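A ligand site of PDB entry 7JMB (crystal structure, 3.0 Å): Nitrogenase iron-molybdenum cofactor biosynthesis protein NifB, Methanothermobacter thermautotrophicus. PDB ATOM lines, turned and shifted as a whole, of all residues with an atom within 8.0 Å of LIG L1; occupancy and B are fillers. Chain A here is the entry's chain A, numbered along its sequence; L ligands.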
ATOM      1  N   HIS A  18     -36.885  20.862  -8.774  1.00  0.00           N
ATOM      2  CA  HIS A  18     -35.905  21.268  -9.772  1.00  0.00           C
ATOM      3  C   HIS A  18     -34.771  22.035  -9.100  1.00  0.00           C
ATOM      4  O   HIS A  18     -34.993  23.123  -8.560  1.00  0.00           O
ATOM      5  CB  HIS A  18     -36.554  22.105 -10.871  1.00  0.00           C
ATOM      6  CG  HIS A  18     -35.671  22.354 -12.049  1.00  0.00           C
ATOM      7  ND1 HIS A  18     -35.800  23.462 -12.860  1.00  0.00           N
ATOM      8  CD2 HIS A  18     -34.661  21.620 -12.573  1.00  0.00           C
ATOM      9  CE1 HIS A  18     -34.891  23.404 -13.825  1.00  0.00           C
ATOM     10  NE2 HIS A  18     -34.187  22.303 -13.677  1.00  0.00           N
ATOM     11  N   PRO A  19     -33.553  21.481  -9.134  1.00  0.00           N
ATOM     12  CA  PRO A  19     -32.437  22.106  -8.417  1.00  0.00           C
ATOM     13  C   PRO A  19     -32.119  23.512  -8.893  1.00  0.00           C
ATOM     14  O   PRO A  19     -31.665  24.338  -8.106  1.00  0.00           O
ATOM     15  CB  PRO A  19     -31.257  21.163  -8.667  1.00  0.00           C
ATOM     16  CG  PRO A  19     -31.787  19.991  -9.408  1.00  0.00           C
ATOM     17  CD  PRO A  19     -33.141  20.308  -9.934  1.00  0.00           C
ATOM     18  N   CYS A  20     -32.343  23.799 -10.183  1.00  0.00           N
ATOM     19  CA  CYS A  20     -32.069  25.124 -10.700  1.00  0.00           C
ATOM     20  C   CYS A  20     -33.054  26.166 -10.187  1.00  0.00           C
ATOM     21  O   CYS A  20     -32.852  27.363 -10.432  1.00  0.00           O
ATOM     22  CB  CYS A  20     -32.084  25.104 -12.227  1.00  0.00           C
ATOM     23  SG  CYS A  20     -30.646  24.290 -12.928  1.00  0.00           S
ATOM     24  N   PHE A  21     -34.117  25.739  -9.516  1.00  0.00           N
ATOM     25  CA  PHE A  21     -35.045  26.628  -8.826  1.00  0.00           C
ATOM     26  C   PHE A  21     -34.951  26.407  -7.327  1.00  0.00           C
ATOM     27  O   PHE A  21     -34.271  25.490  -6.853  1.00  0.00           O
ATOM     28  CB  PHE A  21     -36.478  26.404  -9.340  1.00  0.00           C
ATOM     29  CG  PHE A  21     -36.732  26.976 -10.698  1.00  0.00           C
ATOM     30  CD1 PHE A  21     -37.519  28.109 -10.865  1.00  0.00           C
ATOM     31  CD2 PHE A  21     -36.138  26.420 -11.819  1.00  0.00           C
ATOM     32  CE1 PHE A  21     -37.736  28.645 -12.119  1.00  0.00           C
ATOM     33  CE2 PHE A  21     -36.349  26.947 -13.064  1.00  0.00           C
ATOM     34  CZ  PHE A  21     -37.152  28.062 -13.226  1.00  0.00           C
ATOM     35  N   HIS A  26     -30.647  22.212  -4.700  1.00  0.00           N
ATOM     36  CA  HIS A  26     -29.433  22.358  -5.486  1.00  0.00           C
ATOM     37  C   HIS A  26     -28.328  21.427  -4.988  1.00  0.00           C
ATOM     38  O   HIS A  26     -27.520  20.934  -5.786  1.00  0.00           O
ATOM     39  CB  HIS A  26     -28.974  23.811  -5.447  1.00  0.00           C
ATOM     40  CG  HIS A  26     -28.140  24.232  -6.618  1.00  0.00           C
ATOM     41  ND1 HIS A  26     -27.196  23.412  -7.203  1.00  0.00           N
ATOM     42  CD2 HIS A  26     -28.105  25.392  -7.306  1.00  0.00           C
ATOM     43  CE1 HIS A  26     -26.622  24.065  -8.202  1.00  0.00           C
ATOM     44  NE2 HIS A  26     -27.160  25.266  -8.283  1.00  0.00           N
ATOM     45  N   ARG A  31     -29.161  16.804 -12.021  1.00  0.00           N
ATOM     46  CA  ARG A  31     -29.515  17.186 -13.381  1.00  0.00           C
ATOM     47  C   ARG A  31     -28.476  16.632 -14.337  1.00  0.00           C
ATOM     48  O   ARG A  31     -27.372  16.255 -13.943  1.00  0.00           O
ATOM     49  CB  ARG A  31     -29.602  18.714 -13.516  1.00  0.00           C
ATOM     50  CG  ARG A  31     -28.287  19.411 -13.203  1.00  0.00           C
ATOM     51  CD  ARG A  31     -27.487  19.716 -14.464  1.00  0.00           C
ATOM     52  NE  ARG A  31     -26.098  19.997 -14.138  1.00  0.00           N
ATOM     53  CZ  ARG A  31     -25.663  21.124 -13.585  1.00  0.00           C
ATOM     54  NH1 ARG A  31     -26.512  22.098 -13.288  1.00  0.00           N
ATOM     55  NH2 ARG A  31     -24.372  21.270 -13.320  1.00  0.00           N
ATOM     56  N   HIS A  33     -26.666  17.573 -18.221  1.00  0.00           N
ATOM     57  CA  HIS A  33     -26.448  18.376 -19.410  1.00  0.00           C
ATOM     58  C   HIS A  33     -25.946  17.483 -20.531  1.00  0.00           C
ATOM     59  O   HIS A  33     -25.002  16.700 -20.335  1.00  0.00           O
ATOM     60  CB  HIS A  33     -25.434  19.494 -19.157  1.00  0.00           C
ATOM     61  CG  HIS A  33     -25.956  20.619 -18.331  1.00  0.00           C
ATOM     62  ND1 HIS A  33     -25.149  21.648 -17.889  1.00  0.00           N
ATOM     63  CD2 HIS A  33     -27.204  20.895 -17.876  1.00  0.00           C
ATOM     64  CE1 HIS A  33     -25.873  22.513 -17.195  1.00  0.00           C
ATOM     65  NE2 HIS A  33     -27.122  22.077 -17.179  1.00  0.00           N
ATOM     66  N   PRO A  58     -19.072  28.350 -18.502  1.00  0.00           N
ATOM     67  CA  PRO A  58     -20.474  28.104 -18.895  1.00  0.00           C
ATOM     68  C   PRO A  58     -20.611  27.261 -20.157  1.00  0.00           C
ATOM     69  O   PRO A  58     -21.459  26.364 -20.200  1.00  0.00           O
ATOM     70  CB  PRO A  58     -21.027  29.514 -19.091  1.00  0.00           C
ATOM     71  CG  PRO A  58     -20.206  30.360 -18.174  1.00  0.00           C
ATOM     72  CD  PRO A  58     -18.820  29.779 -18.225  1.00  0.00           C
ATOM     73  N   ALA A  89     -28.117  22.556 -22.387  1.00  0.00           N
ATOM     74  CA  ALA A  89     -27.389  23.813 -22.310  1.00  0.00           C
ATOM     75  C   ALA A  89     -26.055  23.649 -23.020  1.00  0.00           C
ATOM     76  O   ALA A  89     -25.010  23.984 -22.469  1.00  0.00           O
ATOM     77  CB  ALA A  89     -27.180  24.238 -20.852  1.00  0.00           C
ATOM     78  N   CYS A 117     -35.319  20.715 -19.487  1.00  0.00           N
ATOM     79  CA  CYS A 117     -34.982  22.123 -19.378  1.00  0.00           C
ATOM     80  C   CYS A 117     -34.057  22.523 -20.526  1.00  0.00           C
ATOM     81  O   CYS A 117     -33.538  21.682 -21.266  1.00  0.00           O
ATOM     82  CB  CYS A 117     -34.338  22.437 -18.023  1.00  0.00           C
ATOM     83  SG  CYS A 117     -34.367  24.190 -17.584  1.00  0.00           S
ATOM     84  N   MET A 118     -33.850  23.833 -20.662  1.00  0.00           N
ATOM     85  CA  MET A 118     -33.075  24.378 -21.774  1.00  0.00           C
ATOM     86  C   MET A 118     -32.527  25.747 -21.409  1.00  0.00           C
ATOM     87  O   MET A 118     -33.139  26.480 -20.635  1.00  0.00           O
ATOM     88  CB  MET A 118     -33.923  24.497 -23.043  1.00  0.00           C
ATOM     89  CG  MET A 118     -33.964  23.281 -23.931  1.00  0.00           C
ATOM     90  SD  MET A 118     -35.028  23.595 -25.344  1.00  0.00           S
ATOM     91  CE  MET A 118     -34.391  25.184 -25.865  1.00  0.00           C
ATOM     92  N   SER A 119     -31.378  26.067 -21.990  1.00  0.00           N
ATOM     93  CA  SER A 119     -30.742  27.380 -21.849  1.00  0.00           C
ATOM     94  C   SER A 119     -30.632  27.989 -23.244  1.00  0.00           C
ATOM     95  O   SER A 119     -29.821  27.543 -24.055  1.00  0.00           O
ATOM     96  CB  SER A 119     -29.367  27.264 -21.188  1.00  0.00           C
ATOM     97  OG  SER A 119     -28.632  28.458 -21.381  1.00  0.00           O
ATOM     98  N   THR A 141     -34.743  28.779 -19.561  1.00  0.00           N
ATOM     99  CA  THR A 141     -34.111  30.001 -19.066  1.00  0.00           C
ATOM    100  C   THR A 141     -33.531  30.794 -20.234  1.00  0.00           C
ATOM    101  O   THR A 141     -32.946  30.229 -21.162  1.00  0.00           O
ATOM    102  CB  THR A 141     -33.016  29.694 -18.038  1.00  0.00           C
ATOM    103  OG1 THR A 141     -32.213  30.857 -17.829  1.00  0.00           O
ATOM    104  CG2 THR A 141     -32.130  28.556 -18.513  1.00  0.00           C
ATOM    105  N   LYS A 194     -36.956  31.147 -16.603  1.00  0.00           N
ATOM    106  CA  LYS A 194     -35.954  31.800 -15.777  1.00  0.00           C
ATOM    107  C   LYS A 194     -35.181  32.819 -16.599  1.00  0.00           C
ATOM    108  O   LYS A 194     -35.114  32.739 -17.827  1.00  0.00           O
ATOM    109  CB  LYS A 194     -34.987  30.775 -15.165  1.00  0.00           C
ATOM    110  N   ASN A 196     -31.495  34.488 -16.711  1.00  0.00           N
ATOM    111  CA  ASN A 196     -30.099  34.665 -16.343  1.00  0.00           C
ATOM    112  C   ASN A 196     -29.597  35.997 -16.889  1.00  0.00           C
ATOM    113  O   ASN A 196     -29.782  36.299 -18.075  1.00  0.00           O
ATOM    114  CB  ASN A 196     -29.235  33.525 -16.867  1.00  0.00           C
ATOM    115  CG  ASN A 196     -29.517  32.210 -16.161  1.00  0.00           C
ATOM    116  OD1 ASN A 196     -30.439  31.479 -16.531  1.00  0.00           O
ATOM    117  ND2 ASN A 196     -28.734  31.915 -15.134  1.00  0.00           N
ATOM    118  N   LEU A 222     -38.587  33.083 -11.955  1.00  0.00           N
ATOM    119  CA  LEU A 222     -37.361  33.195 -11.186  1.00  0.00           C
ATOM    120  C   LEU A 222     -36.319  33.882 -12.050  1.00  0.00           C
ATOM    121  O   LEU A 222     -36.280  33.711 -13.275  1.00  0.00           O
ATOM    122  CB  LEU A 222     -36.854  31.817 -10.732  1.00  0.00           C
ATOM    123  CG  LEU A 222     -35.671  31.764  -9.777  1.00  0.00           C
ATOM    124  CD1 LEU A 222     -36.044  32.413  -8.451  1.00  0.00           C
ATOM    125  CD2 LEU A 222     -35.196  30.338  -9.551  1.00  0.00           C
ATOM    126  N   ASN A 224     -32.075  34.566 -12.235  1.00  0.00           N
ATOM    127  CA  ASN A 224     -30.785  34.079 -11.741  1.00  0.00           C
ATOM    128  C   ASN A 224     -29.723  35.088 -12.143  1.00  0.00           C
ATOM    129  O   ASN A 224     -29.236  35.075 -13.281  1.00  0.00           O
ATOM    130  CB  ASN A 224     -30.489  32.691 -12.293  1.00  0.00           C
ATOM    131  CG  ASN A 224     -29.241  32.073 -11.681  1.00  0.00           C
ATOM    132  OD1 ASN A 224     -28.590  32.678 -10.816  1.00  0.00           O
ATOM    133  ND2 ASN A 224     -28.898  30.868 -12.123  1.00  0.00           N
ATOM    134  N   ILE A 225     -29.367  35.971 -11.212  1.00  0.00           N
ATOM    135  CA  ILE A 225     -28.283  36.920 -11.445  1.00  0.00           C
ATOM    136  C   ILE A 225     -26.967  36.173 -11.249  1.00  0.00           C
ATOM    137  O   ILE A 225     -26.724  35.591 -10.197  1.00  0.00           O
ATOM    138  CB  ILE A 225     -28.382  38.130 -10.504  1.00  0.00           C
ATOM    139  CG1 ILE A 225     -29.498  39.086 -10.950  1.00  0.00           C
ATOM    140  CG2 ILE A 225     -27.057  38.874 -10.439  1.00  0.00           C
ATOM    141  CD1 ILE A 225     -30.883  38.702 -10.472  1.00  0.00           C
ATOM    142  N   ILE A 226     -26.126  36.187 -12.274  1.00  0.00           N
ATOM    143  CA  ILE A 226     -24.871  35.436 -12.220  1.00  0.00           C
ATOM    144  C   ILE A 226     -23.730  36.442 -12.347  1.00  0.00           C
ATOM    145  O   ILE A 226     -23.845  37.422 -13.088  1.00  0.00           O
ATOM    146  CB  ILE A 226     -24.808  34.370 -13.330  1.00  0.00           C
ATOM    147  N   PHE A 259     -32.844  33.518  -7.711  1.00  0.00           N
ATOM    148  CA  PHE A 259     -32.035  32.343  -7.424  1.00  0.00           C
ATOM    149  C   PHE A 259     -30.664  32.755  -6.890  1.00  0.00           C
ATOM    150  O   PHE A 259     -30.112  33.778  -7.297  1.00  0.00           O
ATOM    151  CB  PHE A 259     -31.888  31.500  -8.686  1.00  0.00           C
ATOM    152  CG  PHE A 259     -31.265  30.156  -8.461  1.00  0.00           C
ATOM    153  CD1 PHE A 259     -31.963  29.156  -7.816  1.00  0.00           C
ATOM    154  CD2 PHE A 259     -29.972  29.903  -8.895  1.00  0.00           C
ATOM    155  CE1 PHE A 259     -31.390  27.912  -7.616  1.00  0.00           C
ATOM    156  CE2 PHE A 259     -29.398  28.669  -8.697  1.00  0.00           C
ATOM    157  CZ  PHE A 259     -30.110  27.680  -8.055  1.00  0.00           C
ATOM    158  N   ALA A 261     -27.857  30.306  -5.950  1.00  0.00           N
ATOM    159  CA  ALA A 261     -26.883  29.228  -5.837  1.00  0.00           C
ATOM    160  C   ALA A 261     -26.393  28.806  -7.216  1.00  0.00           C
ATOM    161  O   ALA A 261     -26.372  27.620  -7.558  1.00  0.00           O
ATOM    162  CB  ALA A 261     -27.457  28.044  -5.070  1.00  0.00           C
ATOM    163  N   CYS A 262     -25.959  29.769  -8.027  1.00  0.00           N
ATOM    164  CA  CYS A 262     -25.564  29.500  -9.405  1.00  0.00           C
ATOM    165  C   CYS A 262     -24.058  29.267  -9.446  1.00  0.00           C
ATOM    166  O   CYS A 262     -23.279  30.206  -9.227  1.00  0.00           O
ATOM    167  CB  CYS A 262     -25.984  30.641 -10.320  1.00  0.00           C
ATOM    168  SG  CYS A 262     -25.609  30.362 -12.084  1.00  0.00           S
ATOM    169  N   THR A 263     -23.655  28.030  -9.721  1.00  0.00           N
ATOM    170  CA  THR A 263     -22.246  27.660  -9.793  1.00  0.00           C
ATOM    171  C   THR A 263     -21.668  27.820 -11.187  1.00  0.00           C
ATOM    172  O   THR A 263     -20.514  27.428 -11.408  1.00  0.00           O
ATOM    173  CB  THR A 263     -22.064  26.216  -9.327  1.00  0.00           C
ATOM    174  OG1 THR A 263     -22.677  25.326 -10.272  1.00  0.00           O
ATOM    175  CG2 THR A 263     -22.705  25.997  -7.972  1.00  0.00           C
ATOM    176  N   GLN A 264     -22.426  28.387 -12.127  1.00  0.00           N
ATOM    177  CA  GLN A 264     -21.998  28.538 -13.518  1.00  0.00           C
ATOM    178  C   GLN A 264     -21.527  27.198 -14.078  1.00  0.00           C
ATOM    179  O   GLN A 264     -20.348  26.962 -14.327  1.00  0.00           O
ATOM    180  CB  GLN A 264     -20.907  29.613 -13.632  1.00  0.00           C
ATOM    181  N   CYS A 265     -22.513  26.328 -14.289  1.00  0.00           N
ATOM    182  CA  CYS A 265     -22.238  24.963 -14.685  1.00  0.00           C
ATOM    183  C   CYS A 265     -21.707  24.898 -16.118  1.00  0.00           C
ATOM    184  O   CYS A 265     -21.895  25.802 -16.931  1.00  0.00           O
ATOM    185  CB  CYS A 265     -23.494  24.120 -14.566  1.00  0.00           C
ATOM    186  SG  CYS A 265     -24.012  23.884 -12.862  1.00  0.00           S
ATOM    187  N   ARG A 266     -21.025  23.792 -16.415  1.00  0.00           N
ATOM    188  CA  ARG A 266     -20.521  23.546 -17.754  1.00  0.00           C
ATOM    189  C   ARG A 266     -21.654  23.042 -18.643  1.00  0.00           C
ATOM    190  O   ARG A 266     -22.819  22.964 -18.244  1.00  0.00           O
ATOM    191  CB  ARG A 266     -19.366  22.537 -17.721  1.00  0.00           C
ATOM    192  N   ALA A 269     -22.146  18.790 -17.561  1.00  0.00           N
ATOM    193  CA  ALA A 269     -22.227  18.368 -16.160  1.00  0.00           C
ATOM    194  C   ALA A 269     -23.378  17.395 -15.953  1.00  0.00           C
ATOM    195  O   ALA A 269     -24.501  17.637 -16.390  1.00  0.00           O
ATOM    196  CB  ALA A 269     -22.384  19.590 -15.263  1.00  0.00           C
ATOM    197  N   PRO A 273     -25.194  19.073  -8.454  1.00  0.00           N
ATOM    198  CA  PRO A 273     -24.177  20.123  -8.600  1.00  0.00           C
ATOM    199  C   PRO A 273     -23.311  20.335  -7.369  1.00  0.00           C
ATOM    200  O   PRO A 273     -22.851  21.461  -7.118  1.00  0.00           O
ATOM    201  CB  PRO A 273     -25.002  21.375  -8.914  1.00  0.00           C
ATOM    202  CG  PRO A 273     -26.324  20.853  -9.421  1.00  0.00           C
ATOM    203  CD  PRO A 273     -26.563  19.598  -8.638  1.00  0.00           C
HETATM  204 FE1  LIG L   1     -28.016  26.462 -14.710  1.00  0.00          FE
HETATM  205 FE2  LIG L   1     -28.015  25.964 -11.658  1.00  0.00          FE
HETATM  206 FE3  LIG L   1     -26.569  28.439 -12.835  1.00  0.00          FE
HETATM  207 FE4  LIG L   1     -25.396  25.639 -13.267  1.00  0.00          FE
HETATM  208  S1  LIG L   1     -25.991  26.794 -11.514  1.00  0.00           S
HETATM  209  S2  LIG L   1     -25.988  27.281 -14.600  1.00  0.00           S
HETATM  210  S3  LIG L   1     -27.420  24.800 -13.408  1.00  0.00           S
HETATM  211  S4  LIG L   1     -28.604  27.627 -12.954  1.00  0.00           S
HETATM  212 FE1  LG2 L   2     -29.615  23.103 -18.032  1.00  0.00          FE
HETATM  213 FE2  LG2 L   2     -32.191  24.480 -17.054  1.00  0.00          FE
HETATM  214 FE3  LG2 L   2     -29.544  26.050 -17.040  1.00  0.00          FE
HETATM  215 FE4  LG2 L   2     -29.975  23.763 -15.023  1.00  0.00          FE
HETATM  216  S1  LG2 L   2     -31.073  25.593 -15.536  1.00  0.00           S
HETATM  217  S2  LG2 L   2     -28.462  24.208 -16.536  1.00  0.00           S
HETATM  218  S3  LG2 L   2     -31.129  22.639 -16.513  1.00  0.00           S
HETATM  219  S4  LG2 L   2     -30.669  24.939 -18.550  1.00  0.00           S
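The backbone NH (N) of Cys 265 sits close to a sulfur (S2) of LIG L1, 3.6 Å away. An iron atom (FE4) of LIG L1 is bound by the side-chain sulfur of Cys 265 (2.3 Å). FE3 of LIG L1 is bound by SG of Cys 262. The guanidinium group of Arg 31 sits close to a sulfur (S3) of LIG L1. A sulfur (S1) of LIG L1 sits close to the backbone NH of Thr 263. A sulfur (S4) of LIG L1 sits close to the side-chain amide nitrogen of Asn 224 (3.4 Å). A sulfur (S1) of LIG L1 sits close to a ring nitrogen (NE2) of His 26 (3.8 Å). SG of Cys 20 is bound to FE4 of LG2 L2 (2.3 Å). A ring nitrogen (NE2) of His 33 lies close to a sulfur (S2) of LG2 L2 (2.6 Å). The backbone NH of Ser 119 lies close to a sulfur (S4) of LG2 L2 (3.7 Å). SG of Cys 117 is bound to FE2 of LG2 L2, at 2.3 Å.
SG of Cys 265 sits close to NH2 of Arg 31 (2.7 Å). The side-chain hydroxyl of Thr 263 lies close to the side-chain sulfur of Cys 265 (3.3 Å). ND2 of Asn 224 sits close to SG of Cys 262 (3.3 Å). SG of Cys 262 lies close to N of Gln 264 (3.7 Å). ND2 of Asn 196 lies close to ND2 of Asn 224. A ring nitrogen (NE2) of His 26 is in hydrogen-bond range of the backbone carbonyl oxygen (O) of Ala 261.
The side-chain sulfur (SG) of Cys 20 sits close to a sulfur (S3) of LIG L1 (3.3 Å). Gln 264 touches LIG L1 (N to S1, 3.95 Å). Of the 28 residues printed, 8 come within 4 Å of LIG L1. The nearest printed residue that does not touch LIG L1 is Ala 261 (4.1 Å).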
